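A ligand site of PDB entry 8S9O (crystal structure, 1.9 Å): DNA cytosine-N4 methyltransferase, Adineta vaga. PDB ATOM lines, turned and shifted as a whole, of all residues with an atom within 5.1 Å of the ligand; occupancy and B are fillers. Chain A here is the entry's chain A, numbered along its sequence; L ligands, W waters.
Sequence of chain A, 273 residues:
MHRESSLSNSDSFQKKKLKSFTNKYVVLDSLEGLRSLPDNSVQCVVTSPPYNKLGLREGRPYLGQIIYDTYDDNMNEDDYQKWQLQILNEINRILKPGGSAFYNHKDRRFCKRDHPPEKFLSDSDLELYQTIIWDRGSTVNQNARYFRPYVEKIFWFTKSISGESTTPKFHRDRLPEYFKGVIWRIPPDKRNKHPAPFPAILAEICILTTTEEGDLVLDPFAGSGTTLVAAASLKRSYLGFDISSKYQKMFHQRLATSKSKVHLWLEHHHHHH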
ATOM      1  N   LEU A  28     -21.148   2.853   6.374  1.00  0.00           N
ATOM      2  CA  LEU A  28     -21.311   1.694   5.521  1.00  0.00           C
ATOM      3  C   LEU A  28     -21.328   2.160   4.076  1.00  0.00           C
ATOM      4  O   LEU A  28     -21.785   3.266   3.780  1.00  0.00           O
ATOM      5  CB  LEU A  28     -22.610   0.950   5.865  1.00  0.00           C
ATOM      6  CG  LEU A  28     -22.974  -0.391   5.229  1.00  0.00           C
ATOM      7  CD1 LEU A  28     -21.929  -1.443   5.539  1.00  0.00           C
ATOM      8  CD2 LEU A  28     -24.335  -0.830   5.730  1.00  0.00           C
ATOM      9  N   ASP A  29     -20.810   1.323   3.182  1.00  0.00           N
ATOM     10  CA  ASP A  29     -20.867   1.637   1.756  1.00  0.00           C
ATOM     11  C   ASP A  29     -22.327   1.791   1.337  1.00  0.00           C
ATOM     12  O   ASP A  29     -23.196   1.024   1.751  1.00  0.00           O
ATOM     13  CB  ASP A  29     -20.187   0.553   0.928  1.00  0.00           C
ATOM     14  CG  ASP A  29     -20.436   0.719  -0.558  1.00  0.00           C
ATOM     15  OD1 ASP A  29     -19.832   1.624  -1.171  1.00  0.00           O
ATOM     16  OD2 ASP A  29     -21.253  -0.042  -1.113  1.00  0.00           O
ATOM     17  N   SER A  30     -22.582   2.800   0.499  1.00  0.00           N
ATOM     18  CA  SER A  30     -23.965   3.164   0.172  1.00  0.00           C
ATOM     19  C   SER A  30     -24.700   2.009  -0.494  1.00  0.00           C
ATOM     20  O   SER A  30     -25.849   1.706  -0.136  1.00  0.00           O
ATOM     21  CB  SER A  30     -23.990   4.396  -0.723  1.00  0.00           C
ATOM     22  OG  SER A  30     -23.380   4.146  -1.976  1.00  0.00           O
ATOM     23  N   SER A  48     -27.363  13.920  -2.240  1.00  0.00           N
ATOM     24  CA  SER A  48     -26.449  14.517  -3.214  1.00  0.00           C
ATOM     25  C   SER A  48     -25.205  13.639  -3.294  1.00  0.00           C
ATOM     26  O   SER A  48     -24.367  13.637  -2.379  1.00  0.00           O
ATOM     27  CB  SER A  48     -26.067  15.942  -2.815  1.00  0.00           C
ATOM     28  OG  SER A  48     -25.217  16.539  -3.782  1.00  0.00           O
ATOM     29  N   PRO A  49     -25.049  12.852  -4.355  1.00  0.00           N
ATOM     30  CA  PRO A  49     -23.952  11.879  -4.420  1.00  0.00           C
ATOM     31  C   PRO A  49     -22.599  12.572  -4.531  1.00  0.00           C
ATOM     32  O   PRO A  49     -22.518  13.736  -4.946  1.00  0.00           O
ATOM     33  CB  PRO A  49     -24.274  11.078  -5.696  1.00  0.00           C
ATOM     34  CG  PRO A  49     -25.105  11.999  -6.520  1.00  0.00           C
ATOM     35  CD  PRO A  49     -25.937  12.758  -5.536  1.00  0.00           C
ATOM     36  N   PRO A  50     -21.530  11.896  -4.154  1.00  0.00           N
ATOM     37  CA  PRO A  50     -20.196  12.480  -4.254  1.00  0.00           C
ATOM     38  C   PRO A  50     -19.699  12.491  -5.692  1.00  0.00           C
ATOM     39  O   PRO A  50     -20.270  11.880  -6.590  1.00  0.00           O
ATOM     40  CB  PRO A  50     -19.336  11.557  -3.389  1.00  0.00           C
ATOM     41  CG  PRO A  50     -20.016  10.230  -3.510  1.00  0.00           C
ATOM     42  CD  PRO A  50     -21.490  10.546  -3.553  1.00  0.00           C
ATOM     43  N   ASN A  52     -16.824  11.159  -6.557  1.00  0.00           N
ATOM     44  CA  ASN A  52     -16.200   9.868  -6.775  1.00  0.00           C
ATOM     45  C   ASN A  52     -16.586   8.919  -5.656  1.00  0.00           C
ATOM     46  O   ASN A  52     -16.924   9.346  -4.540  1.00  0.00           O
ATOM     47  CB  ASN A  52     -14.663   9.993  -6.848  1.00  0.00           C
ATOM     48  CG  ASN A  52     -14.220  11.009  -7.879  1.00  0.00           C
ATOM     49  OD1 ASN A  52     -14.630  10.956  -9.041  1.00  0.00           O
ATOM     50  ND2 ASN A  52     -13.379  11.949  -7.463  1.00  0.00           N
ATOM     51  N   LYS A  53     -16.546   7.624  -5.954  1.00  0.00           N
ATOM     52  CA  LYS A  53     -16.905   6.606  -4.982  1.00  0.00           C
ATOM     53  C   LYS A  53     -15.801   6.457  -3.934  1.00  0.00           C
ATOM     54  O   LYS A  53     -14.638   6.244  -4.273  1.00  0.00           O
ATOM     55  CB  LYS A  53     -17.156   5.269  -5.690  1.00  0.00           C
ATOM     56  CG  LYS A  53     -17.618   4.151  -4.784  1.00  0.00           C
ATOM     57  CD  LYS A  53     -17.737   2.851  -5.563  1.00  0.00           C
ATOM     58  CE  LYS A  53     -18.256   1.727  -4.686  1.00  0.00           C
ATOM     59  NZ  LYS A  53     -17.457   1.600  -3.442  1.00  0.00           N
ATOM     60  N   LEU A  54     -16.184   6.584  -2.661  1.00  0.00           N
ATOM     61  CA  LEU A  54     -15.257   6.514  -1.537  1.00  0.00           C
ATOM     62  C   LEU A  54     -14.134   7.530  -1.681  1.00  0.00           C
ATOM     63  O   LEU A  54     -14.230   8.651  -1.188  1.00  0.00           O
ATOM     64  CB  LEU A  54     -14.687   5.098  -1.386  1.00  0.00           C
ATOM     65  CG  LEU A  54     -14.172   4.690   0.001  1.00  0.00           C
ATOM     66  CD1 LEU A  54     -14.353   3.190   0.214  1.00  0.00           C
ATOM     67  CD2 LEU A  54     -12.709   5.076   0.188  1.00  0.00           C
ATOM     68  N   TRP A  83     -21.938   2.801 -11.570  1.00  0.00           N
ATOM     69  CA  TRP A  83     -22.140   2.761 -10.127  1.00  0.00           C
ATOM     70  C   TRP A  83     -23.420   3.488  -9.716  1.00  0.00           C
ATOM     71  O   TRP A  83     -24.183   2.975  -8.885  1.00  0.00           O
ATOM     72  CB  TRP A  83     -20.917   3.377  -9.431  1.00  0.00           C
ATOM     73  CG  TRP A  83     -21.086   3.606  -7.968  1.00  0.00           C
ATOM     74  CD1 TRP A  83     -21.461   2.687  -7.027  1.00  0.00           C
ATOM     75  CD2 TRP A  83     -20.856   4.829  -7.258  1.00  0.00           C
ATOM     76  NE1 TRP A  83     -21.485   3.269  -5.784  1.00  0.00           N
ATOM     77  CE2 TRP A  83     -21.119   4.581  -5.901  1.00  0.00           C
ATOM     78  CE3 TRP A  83     -20.455   6.105  -7.640  1.00  0.00           C
ATOM     79  CZ2 TRP A  83     -20.995   5.571  -4.922  1.00  0.00           C
ATOM     80  CZ3 TRP A  83     -20.334   7.090  -6.670  1.00  0.00           C
ATOM     81  CH2 TRP A  83     -20.599   6.808  -5.327  1.00  0.00           C
ATOM     82  N   LYS A 106     -24.299  17.582  -8.109  1.00  0.00           N
ATOM     83  CA  LYS A 106     -23.422  18.723  -7.873  1.00  0.00           C
ATOM     84  C   LYS A 106     -22.773  19.210  -9.161  1.00  0.00           C
ATOM     85  O   LYS A 106     -22.557  18.446 -10.110  1.00  0.00           O
ATOM     86  CB  LYS A 106     -22.324  18.360  -6.874  1.00  0.00           C
ATOM     87  CG  LYS A 106     -22.816  18.032  -5.486  1.00  0.00           C
ATOM     88  CD  LYS A 106     -21.642  17.851  -4.547  1.00  0.00           C
ATOM     89  CE  LYS A 106     -22.111  17.315  -3.221  1.00  0.00           C
ATOM     90  NZ  LYS A 106     -22.719  15.963  -3.359  1.00  0.00           N
ATOM     91  N   ASN A 192     -22.424  25.041   8.121  1.00  0.00           N
ATOM     92  CA  ASN A 192     -22.204  23.609   7.961  1.00  0.00           C
ATOM     93  C   ASN A 192     -20.700  23.312   7.864  1.00  0.00           C
ATOM     94  O   ASN A 192     -19.969  23.986   7.137  1.00  0.00           O
ATOM     95  CB  ASN A 192     -22.925  23.091   6.725  1.00  0.00           C
ATOM     96  CG  ASN A 192     -22.993  21.581   6.671  1.00  0.00           C
ATOM     97  OD1 ASN A 192     -21.969  20.907   6.580  1.00  0.00           O
ATOM     98  ND2 ASN A 192     -24.199  21.044   6.742  1.00  0.00           N
ATOM     99  N   HIS A 194     -19.278  20.585   6.661  1.00  0.00           N
ATOM    100  CA  HIS A 194     -18.959  19.672   5.580  1.00  0.00           C
ATOM    101  C   HIS A 194     -18.434  20.445   4.359  1.00  0.00           C
ATOM    102  O   HIS A 194     -18.856  21.571   4.113  1.00  0.00           O
ATOM    103  CB  HIS A 194     -20.201  18.881   5.177  1.00  0.00           C
ATOM    104  CG  HIS A 194     -19.918  17.706   4.301  1.00  0.00           C
ATOM    105  ND1 HIS A 194     -19.778  17.814   2.932  1.00  0.00           N
ATOM    106  CD2 HIS A 194     -19.743  16.392   4.589  1.00  0.00           C
ATOM    107  CE1 HIS A 194     -19.538  16.619   2.418  1.00  0.00           C
ATOM    108  NE2 HIS A 194     -19.509  15.742   3.410  1.00  0.00           N
ATOM    109  N   ALA A 196     -19.049  20.061   1.205  1.00  0.00           N
ATOM    110  CA  ALA A 196     -20.010  20.225   0.119  1.00  0.00           C
ATOM    111  C   ALA A 196     -21.380  19.704   0.528  1.00  0.00           C
ATOM    112  O   ALA A 196     -21.842  18.663   0.052  1.00  0.00           O
ATOM    113  CB  ALA A 196     -19.517  19.522  -1.151  1.00  0.00           C
ATOM    114  N   PRO A 197     -22.059  20.407   1.442  1.00  0.00           N
ATOM    115  CA  PRO A 197     -23.406  19.986   1.881  1.00  0.00           C
ATOM    116  C   PRO A 197     -24.514  20.615   1.037  1.00  0.00           C
ATOM    117  O   PRO A 197     -24.239  21.239   0.014  1.00  0.00           O
ATOM    118  CB  PRO A 197     -23.454  20.481   3.329  1.00  0.00           C
ATOM    119  CG  PRO A 197     -22.581  21.711   3.320  1.00  0.00           C
ATOM    120  CD  PRO A 197     -21.604  21.602   2.177  1.00  0.00           C
ATOM    121  N   PHE A 198     -25.770  20.408   1.428  1.00  0.00           N
ATOM    122  CA  PHE A 198     -26.880  21.236   0.994  1.00  0.00           C
ATOM    123  C   PHE A 198     -27.647  21.724   2.220  1.00  0.00           C
ATOM    124  O   PHE A 198     -27.487  21.176   3.313  1.00  0.00           O
ATOM    125  CB  PHE A 198     -27.820  20.531   0.006  1.00  0.00           C
ATOM    126  CG  PHE A 198     -28.309  19.176   0.425  1.00  0.00           C
ATOM    127  CD1 PHE A 198     -29.046  18.995   1.590  1.00  0.00           C
ATOM    128  CD2 PHE A 198     -28.090  18.076  -0.393  1.00  0.00           C
ATOM    129  CE1 PHE A 198     -29.506  17.738   1.942  1.00  0.00           C
ATOM    130  CE2 PHE A 198     -28.557  16.826  -0.043  1.00  0.00           C
ATOM    131  CZ  PHE A 198     -29.260  16.662   1.126  1.00  0.00           C
ATOM    132  N   ASP A 219     -30.999   9.038   3.304  1.00  0.00           N
ATOM    133  CA  ASP A 219     -29.927   9.664   2.532  1.00  0.00           C
ATOM    134  C   ASP A 219     -28.775   8.681   2.457  1.00  0.00           C
ATOM    135  O   ASP A 219     -28.057   8.498   3.469  1.00  0.00           O
ATOM    136  CB  ASP A 219     -29.475  10.983   3.156  1.00  0.00           C
ATOM    137  CG  ASP A 219     -28.554  11.787   2.247  1.00  0.00           C
ATOM    138  OD1 ASP A 219     -27.841  11.185   1.419  1.00  0.00           O
ATOM    139  OD2 ASP A 219     -28.566  13.034   2.339  1.00  0.00           O
ATOM    140  N   PRO A 220     -28.549   8.024   1.321  1.00  0.00           N
ATOM    141  CA  PRO A 220     -27.450   7.065   1.211  1.00  0.00           C
ATOM    142  C   PRO A 220     -26.069   7.705   1.112  1.00  0.00           C
ATOM    143  O   PRO A 220     -25.083   6.981   0.977  1.00  0.00           O
ATOM    144  CB  PRO A 220     -27.796   6.286  -0.059  1.00  0.00           C
ATOM    145  CG  PRO A 220     -28.583   7.246  -0.883  1.00  0.00           C
ATOM    146  CD  PRO A 220     -29.366   8.084   0.087  1.00  0.00           C
ATOM    147  N   PHE A 221     -25.988   9.037   1.138  1.00  0.00           N
ATOM    148  CA  PHE A 221     -24.733   9.798   1.109  1.00  0.00           C
ATOM    149  C   PHE A 221     -24.799  10.910   2.165  1.00  0.00           C
ATOM    150  O   PHE A 221     -24.643  12.095   1.860  1.00  0.00           O
ATOM    151  CB  PHE A 221     -24.440  10.348  -0.283  1.00  0.00           C
ATOM    152  CG  PHE A 221     -24.306   9.294  -1.345  1.00  0.00           C
ATOM    153  CD1 PHE A 221     -23.208   8.455  -1.383  1.00  0.00           C
ATOM    154  CD2 PHE A 221     -25.285   9.150  -2.324  1.00  0.00           C
ATOM    155  CE1 PHE A 221     -23.079   7.492  -2.366  1.00  0.00           C
ATOM    156  CE2 PHE A 221     -25.169   8.190  -3.305  1.00  0.00           C
ATOM    157  CZ  PHE A 221     -24.069   7.356  -3.334  1.00  0.00           C
ATOM    158  N   ALA A 222     -25.098  10.504   3.400  1.00  0.00           N
ATOM    159  CA  ALA A 222     -25.592  11.425   4.430  1.00  0.00           C
ATOM    160  C   ALA A 222     -24.657  12.614   4.656  1.00  0.00           C
ATOM    161  O   ALA A 222     -25.133  13.739   4.895  1.00  0.00           O
ATOM    162  CB  ALA A 222     -25.806  10.668   5.744  1.00  0.00           C
ATOM    163  N   GLY A 223     -23.348  12.406   4.597  1.00  0.00           N
ATOM    164  CA  GLY A 223     -22.424  13.502   4.860  1.00  0.00           C
ATOM    165  C   GLY A 223     -22.601  14.060   6.259  1.00  0.00           C
ATOM    166  O   GLY A 223     -22.521  13.338   7.251  1.00  0.00           O
ATOM    167  N   SER A 224     -22.850  15.372   6.343  1.00  0.00           N
ATOM    168  CA  SER A 224     -23.066  16.019   7.627  1.00  0.00           C
ATOM    169  C   SER A 224     -24.399  15.639   8.265  1.00  0.00           C
ATOM    170  O   SER A 224     -24.662  16.068   9.394  1.00  0.00           O
ATOM    171  CB  SER A 224     -22.997  17.539   7.470  1.00  0.00           C
ATOM    172  OG  SER A 224     -24.110  18.040   6.741  1.00  0.00           O
ATOM    173  N   GLY A 225     -25.241  14.877   7.572  1.00  0.00           N
ATOM    174  CA  GLY A 225     -26.521  14.480   8.110  1.00  0.00           C
ATOM    175  C   GLY A 225     -27.634  15.468   7.905  1.00  0.00           C
ATOM    176  O   GLY A 225     -28.636  15.408   8.628  1.00  0.00           O
ATOM    177  N   THR A 226     -27.498  16.376   6.943  1.00  0.00           N
ATOM    178  CA  THR A 226     -28.510  17.417   6.713  1.00  0.00           C
ATOM    179  C   THR A 226     -29.902  16.822   6.535  1.00  0.00           C
ATOM    180  O   THR A 226     -30.869  17.297   7.129  1.00  0.00           O
ATOM    181  CB  THR A 226     -28.133  18.255   5.495  1.00  0.00           C
ATOM    182  OG1 THR A 226     -26.846  18.851   5.702  1.00  0.00           O
ATOM    183  CG2 THR A 226     -29.161  19.334   5.259  1.00  0.00           C
ATOM    184  N   PHE A 241     -26.484   6.618   5.272  1.00  0.00           N
ATOM    185  CA  PHE A 241     -25.257   5.876   5.031  1.00  0.00           C
ATOM    186  C   PHE A 241     -24.173   6.849   4.587  1.00  0.00           C
ATOM    187  O   PHE A 241     -24.442   7.780   3.836  1.00  0.00           O
ATOM    188  CB  PHE A 241     -25.422   4.780   3.972  1.00  0.00           C
ATOM    189  CG  PHE A 241     -26.476   3.764   4.301  1.00  0.00           C
ATOM    190  CD1 PHE A 241     -26.410   3.007   5.462  1.00  0.00           C
ATOM    191  CD2 PHE A 241     -27.536   3.549   3.437  1.00  0.00           C
ATOM    192  CE1 PHE A 241     -27.375   2.070   5.754  1.00  0.00           C
ATOM    193  CE2 PHE A 241     -28.508   2.619   3.726  1.00  0.00           C
ATOM    194  CZ  PHE A 241     -28.432   1.872   4.891  1.00  0.00           C
ATOM    195  N   ASP A 242     -22.959   6.611   5.067  1.00  0.00           N
ATOM    196  CA  ASP A 242     -21.790   7.339   4.615  1.00  0.00           C
ATOM    197  C   ASP A 242     -20.571   6.532   5.029  1.00  0.00           C
ATOM    198  O   ASP A 242     -20.603   5.825   6.032  1.00  0.00           O
ATOM    199  CB  ASP A 242     -21.737   8.757   5.186  1.00  0.00           C
ATOM    200  CG  ASP A 242     -20.906   9.704   4.361  1.00  0.00           C
ATOM    201  OD1 ASP A 242     -19.689   9.471   4.224  1.00  0.00           O
ATOM    202  OD2 ASP A 242     -21.465  10.688   3.818  1.00  0.00           O
ATOM    203  N   ILE A 243     -19.490   6.639   4.243  1.00  0.00           N
ATOM    204  CA  ILE A 243     -18.279   5.885   4.555  1.00  0.00           C
ATOM    205  C   ILE A 243     -17.415   6.567   5.590  1.00  0.00           C
ATOM    206  O   ILE A 243     -16.392   5.999   6.001  1.00  0.00           O
ATOM    207  CB  ILE A 243     -17.433   5.607   3.300  1.00  0.00           C
ATOM    208  CG1 ILE A 243     -17.267   6.874   2.460  1.00  0.00           C
ATOM    209  CG2 ILE A 243     -18.045   4.488   2.467  1.00  0.00           C
ATOM    210  CD1 ILE A 243     -15.954   7.595   2.681  1.00  0.00           C
ATOM    211  N   SER A 244     -17.790   7.750   6.054  1.00  0.00           N
ATOM    212  CA  SER A 244     -16.939   8.555   6.923  1.00  0.00           C
ATOM    213  C   SER A 244     -17.436   8.461   8.363  1.00  0.00           C
ATOM    214  O   SER A 244     -18.558   8.891   8.667  1.00  0.00           O
ATOM    215  CB  SER A 244     -16.914  10.009   6.457  1.00  0.00           C
ATOM    216  OG  SER A 244     -16.135  10.810   7.337  1.00  0.00           O
ATOM    217  N   TYR A 247     -17.749  12.139   9.502  1.00  0.00           N
ATOM    218  CA  TYR A 247     -19.028  12.775   9.221  1.00  0.00           C
ATOM    219  C   TYR A 247     -20.142  12.217  10.097  1.00  0.00           C
ATOM    220  O   TYR A 247     -21.067  12.947  10.450  1.00  0.00           O
ATOM    221  CB  TYR A 247     -19.380  12.631   7.735  1.00  0.00           C
ATOM    222  CG  TYR A 247     -18.429  13.365   6.825  1.00  0.00           C
ATOM    223  CD1 TYR A 247     -17.663  14.435   7.293  1.00  0.00           C
ATOM    224  CD2 TYR A 247     -18.278  12.998   5.487  1.00  0.00           C
ATOM    225  CE1 TYR A 247     -16.797  15.110   6.466  1.00  0.00           C
ATOM    226  CE2 TYR A 247     -17.414  13.668   4.651  1.00  0.00           C
ATOM    227  CZ  TYR A 247     -16.676  14.725   5.147  1.00  0.00           C
ATOM    228  OH  TYR A 247     -15.797  15.392   4.309  1.00  0.00           O
HETATM  229  N1  LIG L   1     -25.688  16.423   1.396  1.00  0.00           N
HETATM  230  C1  LIG L   1     -24.664  16.092   2.397  1.00  0.00           C
HETATM  231  C2  LIG L   1     -24.654  17.127   3.513  1.00  0.00           C
HETATM  232  O1  LIG L   1     -25.506  17.961   3.628  1.00  0.00           O
HETATM  233  O2  LIG L   1     -23.639  17.007   4.317  1.00  0.00           O
HETATM  234  C3  LIG L   1     -23.274  15.989   1.770  1.00  0.00           C
HETATM  235  C4  LIG L   1     -23.086  14.763   0.868  1.00  0.00           C
HETATM  236  C5  LIG L   1     -21.667  14.640   0.305  1.00  0.00           C
HETATM  237  N2  LIG L   1     -21.393  15.687  -0.685  1.00  0.00           N
HETATM  238  C6  LIG L   1     -21.388  13.258  -0.288  1.00  0.00           C
HETATM  239  C7  LIG L   1     -20.972  12.226   0.747  1.00  0.00           C
HETATM  240  O3  LIG L   1     -20.835  10.920   0.137  1.00  0.00           O
HETATM  241  C8  LIG L   1     -19.646  12.514   1.466  1.00  0.00           C
HETATM  242  O4  LIG L   1     -19.885  12.803   2.841  1.00  0.00           O
HETATM  243  C9  LIG L   1     -18.836  11.209   1.289  1.00  0.00           C
HETATM  244  O5  LIG L   1     -18.175  10.851   2.495  1.00  0.00           O
HETATM  245  C10 LIG L   1     -19.917  10.207   0.943  1.00  0.00           C
HETATM  246  N3  LIG L   1     -19.465   9.034   0.198  1.00  0.00           N
HETATM  247  C11 LIG L   1     -18.450   8.954  -0.720  1.00  0.00           C
HETATM  248  N4  LIG L   1     -18.266   7.757  -1.217  1.00  0.00           N
HETATM  249  C12 LIG L   1     -19.244   6.983  -0.587  1.00  0.00           C
HETATM  250  C13 LIG L   1     -19.591   5.625  -0.688  1.00  0.00           C
HETATM  251  N5  LIG L   1     -18.990   4.755  -1.491  1.00  0.00           N
HETATM  252  N6  LIG L   1     -20.621   5.185   0.080  1.00  0.00           N
HETATM  253  C14 LIG L   1     -21.236   6.057   0.885  1.00  0.00           C
HETATM  254  N7  LIG L   1     -20.998   7.357   1.053  1.00  0.00           N
HETATM  255  C15 LIG L   1     -19.980   7.764   0.296  1.00  0.00           C
HETATM  256  O   HOH W   1     -26.543  13.570   0.504  1.00  0.00           O
HETATM  257  O   HOH W   2     -24.372  17.911  -0.666  1.00  0.00           O
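The backbone NH (N) of Leu 54 is in hydrogen-bond range of a nitrogen (N4) of the ligand (2.8 Å).
The backbone carbonyl oxygen (O) of Ala 196 sits at hydrogen-bond distance from a nitrogen (N2) of the ligand, 3.1 Å away.
An oxygen (O4) of the ligand is in hydrogen-bond range of a ring nitrogen (NE2) of His 194, at 3.0 Å.
The side-chain hydroxyl (OG) of Ser 224 sits at hydrogen-bond distance from an oxygen (O2) of the ligand (2.7 Å).
An oxygen (O5) of the ligand sits at hydrogen-bond distance from the side-chain carboxylate of Asp 242.
The side-chain hydroxyl (OG1) of Thr 226 is in hydrogen-bond range of an oxygen (O1) of the ligand (2.6 Å).
The side-chain amino group (NZ) of Lys 106 sits close to a nitrogen (N2) of the ligand (3.0 Å).
A nitrogen (N6) of the ligand is in hydrogen-bond range of the backbone NH (N) of Ser 30, 3.1 Å away.
The side-chain carboxylate (OD1) of Asp 29 sits at hydrogen-bond distance from a nitrogen (N5) of the ligand, at 3.3 Å.
O1 of the ligand lies within hydrogen-bond range of N of Phe 198 (3.3 Å).
N of Ser 224 sits at hydrogen-bond distance from O2 of the ligand (2.7 Å).
The side-chain carboxylate of Asp 242 is in hydrogen-bond range of the backbone NH of Gly 223 (2.7 Å).
N of Tyr 247 lies within hydrogen-bond range of OG of Ser 244 (3.0 Å).
The backbone carbonyl oxygen (O) of Phe 198 sits close to the side-chain hydroxyl (OG1) of Thr 226, 3.4 Å away.
N of Ser 244 sits at hydrogen-bond distance from OD1 of Asp 242 (3.1 Å).
N of Leu 28 lies within hydrogen-bond range of O of Asp 242.
N of Ala 222 lies within hydrogen-bond range of OD1 of Asp 219 (3.5 Å).
The side-chain carboxylate of Asp 29 is in salt-bridge range of the side-chain amino group of Lys 53 (3.3 Å).
The backbone NH (N) of Ala 222 lies within hydrogen-bond range of the backbone carbonyl oxygen (O) of Phe 241, 2.8 Å away.
Water W2 lies within hydrogen-bond range of the backbone carbonyl oxygen (O) of Ala 196 (2.7 Å), a nitrogen (N1) of the ligand (2.9 Å) and the backbone carbonyl oxygen (O) of Pro 197 (3.4 Å).
Water W1 lies within hydrogen-bond range of O of Phe 221 (2.8 Å), OD2 of Asp 219 (2.8 Å), N of Ser 48 (2.9 Å) and N1 of the ligand (3.1 Å).
Ser 48 touches the ligand (O to C6, 3.7 Å).
Pro 50 touches the ligand (CG to C11, 3.4 Å).
Asn 52 touches the ligand.
CG of Lys 53 touches N5 of the ligand (3.6 Å).
Pro 197 touches the ligand.
Pro 220 touches the ligand.
O of Phe 221 touches C4 of the ligand, at 3.2 Å.
O of Ala 222 touches C1 of the ligand (3.5 Å).
Gly 223 touches the ligand.
Ile 243 touches the ligand.
Tyr 247 touches the ligand.
Hydrophobic or aromatic side chains within 4 Å of the ligand: Pro 50, His 194, Pro 197, Phe 198, Phe 221, Ile 243 and Tyr 247.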
